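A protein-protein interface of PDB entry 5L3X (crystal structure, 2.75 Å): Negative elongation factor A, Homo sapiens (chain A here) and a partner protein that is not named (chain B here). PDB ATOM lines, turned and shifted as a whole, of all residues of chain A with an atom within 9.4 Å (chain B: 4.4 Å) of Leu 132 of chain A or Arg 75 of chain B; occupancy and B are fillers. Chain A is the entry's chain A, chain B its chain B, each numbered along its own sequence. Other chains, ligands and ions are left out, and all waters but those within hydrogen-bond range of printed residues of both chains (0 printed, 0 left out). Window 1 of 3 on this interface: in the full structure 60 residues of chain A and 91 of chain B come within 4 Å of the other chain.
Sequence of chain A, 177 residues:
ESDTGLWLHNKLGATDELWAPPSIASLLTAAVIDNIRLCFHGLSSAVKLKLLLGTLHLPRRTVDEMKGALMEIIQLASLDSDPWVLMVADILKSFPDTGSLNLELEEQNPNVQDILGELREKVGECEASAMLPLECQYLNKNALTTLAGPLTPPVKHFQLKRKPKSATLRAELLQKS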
ATOM      1  N   CYS A 126       6.923   1.897 -12.164  1.00  0.00           N
ATOM      2  CA  CYS A 126       6.462   3.197 -11.688  1.00  0.00           C
ATOM      3  C   CYS A 126       5.473   3.828 -12.663  1.00  0.00           C
ATOM      4  O   CYS A 126       5.549   5.022 -12.952  1.00  0.00           O
ATOM      5  CB  CYS A 126       7.649   4.135 -11.460  1.00  0.00           C
ATOM      6  SG  CYS A 126       8.783   3.599 -10.156  1.00  0.00           S
ATOM      7  N   GLU A 127       4.548   3.018 -13.165  1.00  0.00           N
ATOM      8  CA  GLU A 127       3.508   3.506 -14.061  1.00  0.00           C
ATOM      9  C   GLU A 127       2.336   4.066 -13.263  1.00  0.00           C
ATOM     10  O   GLU A 127       1.504   4.802 -13.794  1.00  0.00           O
ATOM     11  CB  GLU A 127       3.026   2.391 -14.993  1.00  0.00           C
ATOM     12  CG  GLU A 127       2.490   1.165 -14.271  1.00  0.00           C
ATOM     13  CD  GLU A 127       1.892   0.143 -15.220  1.00  0.00           C
ATOM     14  OE1 GLU A 127       1.166   0.551 -16.152  1.00  0.00           O
ATOM     15  OE2 GLU A 127       2.150  -1.066 -15.037  1.00  0.00           O
ATOM     16  N   ALA A 128       2.278   3.709 -11.984  1.00  0.00           N
ATOM     17  CA  ALA A 128       1.231   4.202 -11.097  1.00  0.00           C
ATOM     18  C   ALA A 128       1.484   5.655 -10.712  1.00  0.00           C
ATOM     19  O   ALA A 128       2.441   5.957  -9.994  1.00  0.00           O
ATOM     20  CB  ALA A 128       1.135   3.330  -9.854  1.00  0.00           C
ATOM     21  N   SER A 129       0.620   6.544 -11.200  1.00  0.00           N
ATOM     22  CA  SER A 129       0.713   7.980 -10.933  1.00  0.00           C
ATOM     23  C   SER A 129       2.066   8.558 -11.346  1.00  0.00           C
ATOM     24  O   SER A 129       2.643   9.383 -10.636  1.00  0.00           O
ATOM     25  CB  SER A 129       0.451   8.270  -9.452  1.00  0.00           C
ATOM     26  OG  SER A 129      -0.839   7.830  -9.068  1.00  0.00           O
ATOM     27  N   ALA A 130       2.560   8.120 -12.500  1.00  0.00           N
ATOM     28  CA  ALA A 130       3.852   8.573 -13.006  1.00  0.00           C
ATOM     29  C   ALA A 130       3.811  10.058 -13.357  1.00  0.00           C
ATOM     30  O   ALA A 130       2.794  10.568 -13.824  1.00  0.00           O
ATOM     31  CB  ALA A 130       4.266   7.747 -14.219  1.00  0.00           C
ATOM     32  N   MET A 131       4.925  10.744 -13.118  1.00  0.00           N
ATOM     33  CA  MET A 131       5.032  12.158 -13.438  1.00  0.00           C
ATOM     34  C   MET A 131       4.911  12.382 -14.942  1.00  0.00           C
ATOM     35  O   MET A 131       5.463  11.630 -15.748  1.00  0.00           O
ATOM     36  CB  MET A 131       6.349  12.734 -12.910  1.00  0.00           C
ATOM     37  CG  MET A 131       7.592  11.998 -13.368  1.00  0.00           C
ATOM     38  SD  MET A 131       9.052  12.524 -12.446  1.00  0.00           S
ATOM     39  CE  MET A 131      10.259  11.327 -12.996  1.00  0.00           C
ATOM     40  N   LEU A 132       4.169  13.420 -15.311  1.00  0.00           N
ATOM     41  CA  LEU A 132       3.899  13.713 -16.710  1.00  0.00           C
ATOM     42  C   LEU A 132       4.933  14.704 -17.249  1.00  0.00           C
ATOM     43  O   LEU A 132       5.649  15.336 -16.475  1.00  0.00           O
ATOM     44  CB  LEU A 132       2.479  14.261 -16.869  1.00  0.00           C
ATOM     45  CG  LEU A 132       1.293  13.330 -16.572  1.00  0.00           C
ATOM     46  CD1 LEU A 132       1.062  13.154 -15.075  1.00  0.00           C
ATOM     47  CD2 LEU A 132       0.026  13.845 -17.241  1.00  0.00           C
ATOM     48  N   PRO A 133       5.036  14.826 -18.582  1.00  0.00           N
ATOM     49  CA  PRO A 133       5.913  15.847 -19.168  1.00  0.00           C
ATOM     50  C   PRO A 133       5.458  17.267 -18.834  1.00  0.00           C
ATOM     51  O   PRO A 133       4.351  17.459 -18.337  1.00  0.00           O
ATOM     52  CB  PRO A 133       5.806  15.578 -20.672  1.00  0.00           C
ATOM     53  CG  PRO A 133       5.444  14.145 -20.762  1.00  0.00           C
ATOM     54  CD  PRO A 133       4.536  13.889 -19.601  1.00  0.00           C
ATOM     55  N   LEU A 134       6.306  18.252 -19.114  1.00  0.00           N
ATOM     56  CA  LEU A 134       6.030  19.627 -18.709  1.00  0.00           C
ATOM     57  C   LEU A 134       4.922  20.283 -19.529  1.00  0.00           C
ATOM     58  O   LEU A 134       4.203  21.145 -19.019  1.00  0.00           O
ATOM     59  CB  LEU A 134       7.308  20.467 -18.794  1.00  0.00           C
ATOM     60  CG  LEU A 134       8.412  20.123 -17.786  1.00  0.00           C
ATOM     61  CD1 LEU A 134       9.705  20.844 -18.129  1.00  0.00           C
ATOM     62  CD2 LEU A 134       7.977  20.443 -16.361  1.00  0.00           C
ATOM     63  N   GLU A 135       4.778  19.876 -20.790  1.00  0.00           N
ATOM     64  CA  GLU A 135       3.793  20.503 -21.671  1.00  0.00           C
ATOM     65  C   GLU A 135       2.379  20.272 -21.158  1.00  0.00           C
ATOM     66  O   GLU A 135       1.490  21.086 -21.416  1.00  0.00           O
ATOM     67  CB  GLU A 135       3.922  19.991 -23.116  1.00  0.00           C
ATOM     68  CG  GLU A 135       3.513  18.541 -23.335  1.00  0.00           C
ATOM     69  CD  GLU A 135       4.702  17.609 -23.493  1.00  0.00           C
ATOM     70  OE1 GLU A 135       5.810  17.969 -23.043  1.00  0.00           O
ATOM     71  OE2 GLU A 135       4.529  16.517 -24.075  1.00  0.00           O
ATOM     72  N   CYS A 136       2.183  19.173 -20.423  1.00  0.00           N
ATOM     73  CA  CYS A 136       0.876  18.816 -19.864  1.00  0.00           C
ATOM     74  C   CYS A 136       0.352  19.864 -18.886  1.00  0.00           C
ATOM     75  O   CYS A 136      -0.852  19.972 -18.663  1.00  0.00           O
ATOM     76  CB  CYS A 136       0.950  17.462 -19.163  1.00  0.00           C
ATOM     77  SG  CYS A 136       1.453  16.090 -20.230  1.00  0.00           S
ATOM     78  N   GLN A 137       1.266  20.635 -18.309  1.00  0.00           N
ATOM     79  CA  GLN A 137       0.907  21.671 -17.355  1.00  0.00           C
ATOM     80  C   GLN A 137       0.235  22.855 -18.041  1.00  0.00           C
ATOM     81  O   GLN A 137      -0.401  23.687 -17.387  1.00  0.00           O
ATOM     82  CB  GLN A 137       2.153  22.130 -16.587  1.00  0.00           C
ATOM     83  CG  GLN A 137       2.924  20.983 -15.961  1.00  0.00           C
ATOM     84  CD  GLN A 137       4.113  21.438 -15.138  1.00  0.00           C
ATOM     85  OE1 GLN A 137       4.687  20.656 -14.379  1.00  0.00           O
ATOM     86  NE2 GLN A 137       4.491  22.706 -15.284  1.00  0.00           N
ATOM     87  N   TYR A 138       0.369  22.917 -19.363  1.00  0.00           N
ATOM     88  CA  TYR A 138      -0.174  24.025 -20.153  1.00  0.00           C
ATOM     89  C   TYR A 138      -1.478  23.684 -20.877  1.00  0.00           C
ATOM     90  O   TYR A 138      -2.007  24.519 -21.613  1.00  0.00           O
ATOM     91  CB  TYR A 138       0.845  24.484 -21.205  1.00  0.00           C
ATOM     92  CG  TYR A 138       2.141  25.064 -20.680  1.00  0.00           C
ATOM     93  CD1 TYR A 138       3.195  24.240 -20.308  1.00  0.00           C
ATOM     94  CD2 TYR A 138       2.328  26.438 -20.603  1.00  0.00           C
ATOM     95  CE1 TYR A 138       4.387  24.766 -19.849  1.00  0.00           C
ATOM     96  CE2 TYR A 138       3.521  26.975 -20.146  1.00  0.00           C
ATOM     97  CZ  TYR A 138       4.544  26.136 -19.769  1.00  0.00           C
ATOM     98  OH  TYR A 138       5.731  26.666 -19.313  1.00  0.00           O
ATOM     99  N   LEU A 139      -1.984  22.465 -20.688  1.00  0.00           N
ATOM    100  CA  LEU A 139      -3.080  21.969 -21.521  1.00  0.00           C
ATOM    101  C   LEU A 139      -4.450  22.016 -20.836  1.00  0.00           C
ATOM    102  O   LEU A 139      -4.560  21.815 -19.629  1.00  0.00           O
ATOM    103  CB  LEU A 139      -2.779  20.541 -21.972  1.00  0.00           C
ATOM    104  CG  LEU A 139      -1.425  20.303 -22.660  1.00  0.00           C
ATOM    105  CD1 LEU A 139      -1.244  18.833 -23.031  1.00  0.00           C
ATOM    106  CD2 LEU A 139      -1.285  21.183 -23.890  1.00  0.00           C
ATOM    107  N   ALA A 143      -7.536  18.257 -24.040  1.00  0.00           N
ATOM    108  CA  ALA A 143      -6.264  18.000 -24.706  1.00  0.00           C
ATOM    109  C   ALA A 143      -5.372  17.123 -23.817  1.00  0.00           C
ATOM    110  O   ALA A 143      -4.694  16.208 -24.297  1.00  0.00           O
ATOM    111  CB  ALA A 143      -5.560  19.311 -25.054  1.00  0.00           C
ATOM    112  N   LEU A 144      -5.397  17.398 -22.517  1.00  0.00           N
ATOM    113  CA  LEU A 144      -4.621  16.631 -21.551  1.00  0.00           C
ATOM    114  C   LEU A 144      -5.040  15.165 -21.527  1.00  0.00           C
ATOM    115  O   LEU A 144      -4.195  14.272 -21.540  1.00  0.00           O
ATOM    116  CB  LEU A 144      -4.757  17.236 -20.146  1.00  0.00           C
ATOM    117  CG  LEU A 144      -3.977  16.484 -19.058  1.00  0.00           C
ATOM    118  CD1 LEU A 144      -2.491  16.475 -19.360  1.00  0.00           C
ATOM    119  CD2 LEU A 144      -4.230  17.055 -17.670  1.00  0.00           C
ATOM    120  N   THR A 145      -6.349  14.921 -21.496  1.00  0.00           N
ATOM    121  CA  THR A 145      -6.871  13.559 -21.410  1.00  0.00           C
ATOM    122  C   THR A 145      -6.626  12.785 -22.704  1.00  0.00           C
ATOM    123  O   THR A 145      -6.323  11.597 -22.676  1.00  0.00           O
ATOM    124  CB  THR A 145      -8.375  13.554 -21.092  1.00  0.00           C
ATOM    125  OG1 THR A 145      -8.603  14.199 -19.830  1.00  0.00           O
ATOM    126  CG2 THR A 145      -8.905  12.129 -21.034  1.00  0.00           C
ATOM    127  N   LEU A 147      -4.110  13.233 -24.686  1.00  0.00           N
ATOM    128  CA  LEU A 147      -2.678  12.987 -24.779  1.00  0.00           C
ATOM    129  C   LEU A 147      -2.151  12.014 -23.718  1.00  0.00           C
ATOM    130  O   LEU A 147      -1.362  11.125 -24.035  1.00  0.00           O
ATOM    131  CB  LEU A 147      -1.917  14.312 -24.686  1.00  0.00           C
ATOM    132  CG  LEU A 147      -0.398  14.235 -24.859  1.00  0.00           C
ATOM    133  CD1 LEU A 147      -0.036  13.917 -26.303  1.00  0.00           C
ATOM    134  CD2 LEU A 147       0.269  15.522 -24.397  1.00  0.00           C
ATOM    135  N   ALA A 148      -2.581  12.171 -22.469  1.00  0.00           N
ATOM    136  CA  ALA A 148      -1.996  11.399 -21.369  1.00  0.00           C
ATOM    137  C   ALA A 148      -3.010  10.591 -20.565  1.00  0.00           C
ATOM    138  O   ALA A 148      -2.637   9.892 -19.622  1.00  0.00           O
ATOM    139  CB  ALA A 148      -1.226  12.328 -20.434  1.00  0.00           C
ATOM    140  N   GLY A 149      -4.287  10.685 -20.922  1.00  0.00           N
ATOM    141  CA  GLY A 149      -5.319   9.966 -20.191  1.00  0.00           C
ATOM    142  C   GLY A 149      -5.787  10.728 -18.965  1.00  0.00           C
ATOM    143  O   GLY A 149      -5.255  11.792 -18.663  1.00  0.00           O
ATOM    144  N   PRO A 150      -6.785  10.187 -18.248  1.00  0.00           N
ATOM    145  CA  PRO A 150      -7.307  10.827 -17.034  1.00  0.00           C
ATOM    146  C   PRO A 150      -6.218  10.981 -15.977  1.00  0.00           C
ATOM    147  O   PRO A 150      -5.372  10.099 -15.850  1.00  0.00           O
ATOM    148  CB  PRO A 150      -8.394   9.852 -16.550  1.00  0.00           C
ATOM    149  CG  PRO A 150      -8.668   8.957 -17.705  1.00  0.00           C
ATOM    150  CD  PRO A 150      -7.393   8.866 -18.475  1.00  0.00           C
ATOM    151  N   LEU A 151      -6.224  12.087 -15.244  1.00  0.00           N
ATOM    152  CA  LEU A 151      -5.281  12.251 -14.148  1.00  0.00           C
ATOM    153  C   LEU A 151      -5.742  11.449 -12.944  1.00  0.00           C
ATOM    154  O   LEU A 151      -6.932  11.412 -12.627  1.00  0.00           O
ATOM    155  CB  LEU A 151      -5.129  13.720 -13.748  1.00  0.00           C
ATOM    156  CG  LEU A 151      -4.435  14.702 -14.687  1.00  0.00           C
ATOM    157  CD1 LEU A 151      -4.182  16.012 -13.937  1.00  0.00           C
ATOM    158  CD2 LEU A 151      -3.145  14.116 -15.236  1.00  0.00           C
ATOM    159  N   THR A 152      -4.796  10.803 -12.276  1.00  0.00           N
ATOM    160  CA  THR A 152      -5.089  10.158 -11.012  1.00  0.00           C
ATOM    161  C   THR A 152      -5.329  11.214  -9.941  1.00  0.00           C
ATOM    162  O   THR A 152      -4.492  12.091  -9.734  1.00  0.00           O
ATOM    163  CB  THR A 152      -3.946   9.238 -10.570  1.00  0.00           C
ATOM    164  OG1 THR A 152      -3.703   8.252 -11.582  1.00  0.00           O
ATOM    165  CG2 THR A 152      -4.302   8.565  -9.263  1.00  0.00           C
ATOM    166  N   GLU B  32       8.131  12.908  -8.664  1.00  0.00           N
ATOM    167  CA  GLU B  32       8.218  14.320  -9.017  1.00  0.00           C
ATOM    168  C   GLU B  32       8.602  15.154  -7.797  1.00  0.00           C
ATOM    169  O   GLU B  32       9.148  16.249  -7.926  1.00  0.00           O
ATOM    170  CB  GLU B  32       6.891  14.805  -9.609  1.00  0.00           C
ATOM    171  CG  GLU B  32       6.962  16.171 -10.271  1.00  0.00           C
ATOM    172  CD  GLU B  32       5.721  16.492 -11.085  1.00  0.00           C
ATOM    173  OE1 GLU B  32       5.681  17.578 -11.701  1.00  0.00           O
ATOM    174  OE2 GLU B  32       4.789  15.658 -11.108  1.00  0.00           O
ATOM    175  N   LEU B  35      12.351  15.167  -7.338  1.00  0.00           N
ATOM    176  CA  LEU B  35      12.941  15.433  -8.643  1.00  0.00           C
ATOM    177  C   LEU B  35      14.007  16.522  -8.574  1.00  0.00           C
ATOM    178  O   LEU B  35      15.071  16.396  -9.176  1.00  0.00           O
ATOM    179  CB  LEU B  35      11.855  15.831  -9.641  1.00  0.00           C
ATOM    180  CG  LEU B  35      12.313  16.173 -11.057  1.00  0.00           C
ATOM    181  CD1 LEU B  35      12.998  14.980 -11.701  1.00  0.00           C
ATOM    182  CD2 LEU B  35      11.130  16.637 -11.893  1.00  0.00           C
ATOM    183  N   SER B  71       6.167   8.124 -20.279  1.00  0.00           N
ATOM    184  CA  SER B  71       5.984   9.561 -20.164  1.00  0.00           C
ATOM    185  C   SER B  71       6.867  10.128 -19.060  1.00  0.00           C
ATOM    186  O   SER B  71       7.280  11.287 -19.115  1.00  0.00           O
ATOM    187  CB  SER B  71       4.516   9.904 -19.883  1.00  0.00           C
ATOM    188  OG  SER B  71       4.165   9.566 -18.550  1.00  0.00           O
ATOM    189  N   ALA B  72       7.151   9.305 -18.056  1.00  0.00           N
ATOM    190  CA  ALA B  72       7.960   9.737 -16.923  1.00  0.00           C
ATOM    191  C   ALA B  72       9.410   9.973 -17.340  1.00  0.00           C
ATOM    192  O   ALA B  72      10.116  10.778 -16.727  1.00  0.00           O
ATOM    193  CB  ALA B  72       7.890   8.712 -15.796  1.00  0.00           C
ATOM    194  N   VAL B  73       9.848   9.277 -18.385  1.00  0.00           N
ATOM    195  CA  VAL B  73      11.208   9.438 -18.884  1.00  0.00           C
ATOM    196  C   VAL B  73      11.285  10.667 -19.777  1.00  0.00           C
ATOM    197  O   VAL B  73      12.288  11.386 -19.781  1.00  0.00           O
ATOM    198  CB  VAL B  73      11.686   8.192 -19.655  1.00  0.00           C
ATOM    199  CG1 VAL B  73      13.113   8.387 -20.159  1.00  0.00           C
ATOM    200  CG2 VAL B  73      11.603   6.965 -18.763  1.00  0.00           C
ATOM    201  N   ARG B  74      10.213  10.911 -20.524  1.00  0.00           N
ATOM    202  CA  ARG B  74      10.107  12.113 -21.346  1.00  0.00           C
ATOM    203  C   ARG B  74      10.204  13.354 -20.461  1.00  0.00           C
ATOM    204  O   ARG B  74      10.787  14.364 -20.852  1.00  0.00           O
ATOM    205  CB  ARG B  74       8.798  12.107 -22.138  1.00  0.00           C
ATOM    206  CG  ARG B  74       8.652  13.244 -23.126  1.00  0.00           C
ATOM    207  CD  ARG B  74       7.386  13.077 -23.954  1.00  0.00           C
ATOM    208  NE  ARG B  74       6.984  14.317 -24.619  1.00  0.00           N
ATOM    209  CZ  ARG B  74       7.402  14.691 -25.823  1.00  0.00           C
ATOM    210  NH1 ARG B  74       8.246  13.925 -26.501  1.00  0.00           N
ATOM    211  NH2 ARG B  74       6.981  15.832 -26.350  1.00  0.00           N
ATOM    212  N   ARG B  75       9.643  13.261 -19.259  1.00  0.00           N
ATOM    213  CA  ARG B  75       9.755  14.332 -18.280  1.00  0.00           C
ATOM    214  C   ARG B  75      11.211  14.545 -17.872  1.00  0.00           C
ATOM    215  O   ARG B  75      11.690  15.678 -17.825  1.00  0.00           O
ATOM    216  CB  ARG B  75       8.906  14.026 -17.048  1.00  0.00           C
ATOM    217  CG  ARG B  75       9.114  14.997 -15.899  1.00  0.00           C
ATOM    218  CD  ARG B  75       8.722  16.415 -16.286  1.00  0.00           C
ATOM    219  NE  ARG B  75       8.859  17.343 -15.166  1.00  0.00           N
ATOM    220  CZ  ARG B  75       7.958  17.483 -14.197  1.00  0.00           C
ATOM    221  NH1 ARG B  75       6.851  16.754 -14.204  1.00  0.00           N
ATOM    222  NH2 ARG B  75       8.166  18.351 -13.216  1.00  0.00           N
ATOM    223  N   ILE B  76      11.908  13.449 -17.577  1.00  0.00           N
ATOM    224  CA  ILE B  76      13.309  13.520 -17.184  1.00  0.00           C
ATOM    225  C   ILE B  76      14.159  14.141 -18.288  1.00  0.00           C
ATOM    226  O   ILE B  76      15.024  14.976 -18.020  1.00  0.00           O
ATOM    227  CB  ILE B  76      13.876  12.122 -16.828  1.00  0.00           C
ATOM    228  CG1 ILE B  76      13.106  11.515 -15.655  1.00  0.00           C
ATOM    229  CG2 ILE B  76      15.366  12.207 -16.496  1.00  0.00           C
ATOM    230  CD1 ILE B  76      13.403  10.048 -15.420  1.00  0.00           C
ATOM    231  N   ALA B  77      13.900  13.734 -19.529  1.00  0.00           N
ATOM    232  CA  ALA B  77      14.659  14.233 -20.667  1.00  0.00           C
ATOM    233  C   ALA B  77      14.478  15.741 -20.811  1.00  0.00           C
ATOM    234  O   ALA B  77      15.431  16.467 -21.096  1.00  0.00           O
ATOM    235  CB  ALA B  77      14.241  13.520 -21.935  1.00  0.00           C
ATOM    236  N   GLN B  78      13.252  16.207 -20.599  1.00  0.00           N
ATOM    237  CA  GLN B  78      12.939  17.629 -20.702  1.00  0.00           C
ATOM    238  C   GLN B  78      13.587  18.423 -19.569  1.00  0.00           C
ATOM    239  O   GLN B  78      13.989  19.570 -19.759  1.00  0.00           O
ATOM    240  CB  GLN B  78      11.422  17.841 -20.704  1.00  0.00           C
ATOM    241  CG  GLN B  78      10.745  17.338 -21.969  1.00  0.00           C
ATOM    242  CD  GLN B  78       9.239  17.211 -21.827  1.00  0.00           C
ATOM    243  OE1 GLN B  78       8.682  17.422 -20.750  1.00  0.00           O
ATOM    244  NE2 GLN B  78       8.574  16.862 -22.918  1.00  0.00           N
ATOM    245  N   GLU B  79      13.686  17.813 -18.394  1.00  0.00           N
ATOM    246  CA  GLU B  79      14.350  18.452 -17.267  1.00  0.00           C
ATOM    247  C   GLU B  79      15.846  18.638 -17.545  1.00  0.00           C
ATOM    248  O   GLU B  79      16.440  19.654 -17.170  1.00  0.00           O
ATOM    249  CB  GLU B  79      14.141  17.636 -15.992  1.00  0.00           C
ATOM    250  CG  GLU B  79      12.720  17.673 -15.460  1.00  0.00           C
ATOM    251  CD  GLU B  79      12.368  19.000 -14.837  1.00  0.00           C
ATOM    252  OE1 GLU B  79      13.299  19.768 -14.503  1.00  0.00           O
ATOM    253  OE2 GLU B  79      11.161  19.278 -14.682  1.00  0.00           O
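NH1 of Arg 75 of chain B sits at hydrogen-bond distance from O of Leu 132 of chain A.
The backbone NH (N) of Leu 134 of chain A sits at hydrogen-bond distance from the side-chain amide oxygen (OE1) of Gln 78 of chain B, 3.0 Å away.
The side-chain carboxylate of Glu 135 of chain A lies within salt-bridge range of the guanidinium group of Arg 74 of chain B (3.3 Å).
The side-chain amide nitrogen (NE2) of Gln 78 of chain B is in hydrogen-bond range of the side-chain carboxylate (OE1) of Glu 135 of chain A (3.0 Å).
SG of Cys 136 of chain A sits close to O of Pro 133 of chain A, at 3.7 Å.
NH1 of Arg 75 of chain B lies within salt-bridge range of OE1 of Glu 32 of chain B (2.9 Å).
The guanidinium group of Arg 74 of chain B lies close to the side-chain amide nitrogen of Gln 78 of chain B.
The side-chain carboxylate of Glu 79 of chain B is in salt-bridge range of the guanidinium group of Arg 75 of chain B, at 3.0 Å.
Among the printed residues, merely in contact across the chains: Met 131 of chain A with Ala 72 of chain B, Pro 133 of chain A with Gln 78 of chain B, Leu 134 of chain A with Arg 75 of chain B, Met 131 of chain A with Ser 71 of chain B, Met 131 of chain A with Glu 32 of chain B, Pro 133 of chain A with Ser 71 of chain B, Leu 134 of chain A with Glu 79 of chain B, Pro 133 of chain A with Arg 74 of chain B and Met 131 of chain A with Ile 76 of chain B.
Leu 132 of chain A touches just one residue of chain B: Arg 75 (2.9 Å).
Arg 75 of chain B touches two residues of chain A.
Gln 78 of chain B touches just these residues of chain A: Pro 133 (3.4 Å), Leu 134 (3.0 Å) and Glu 135 (3.0 Å).
Printed residues of chain A within 4 Å of Glu 32 of chain B: Met 131.
Printed residues of chain B within 4 Å of Glu 135 of chain A: Arg 74 and Gln 78.
Printed residues of chain A within 4 Å of Ile 76 of chain B: Met 131.
The nearest printed residue of chain B that does not touch Leu 132 of chain A is Ser 71 of chain B (4.5 Å).
The nearest residue of chain A that does not touch Arg 75 of chain B is Pro 133 of chain A (4.1 Å).
Of the 23 printed residues of chain A, 5 touch a printed residue of chain B.
Hydrophobic or aromatic side chains of chain A within 4 Å of the printed part of chain B: Met 131, Pro 133 and Leu 134.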
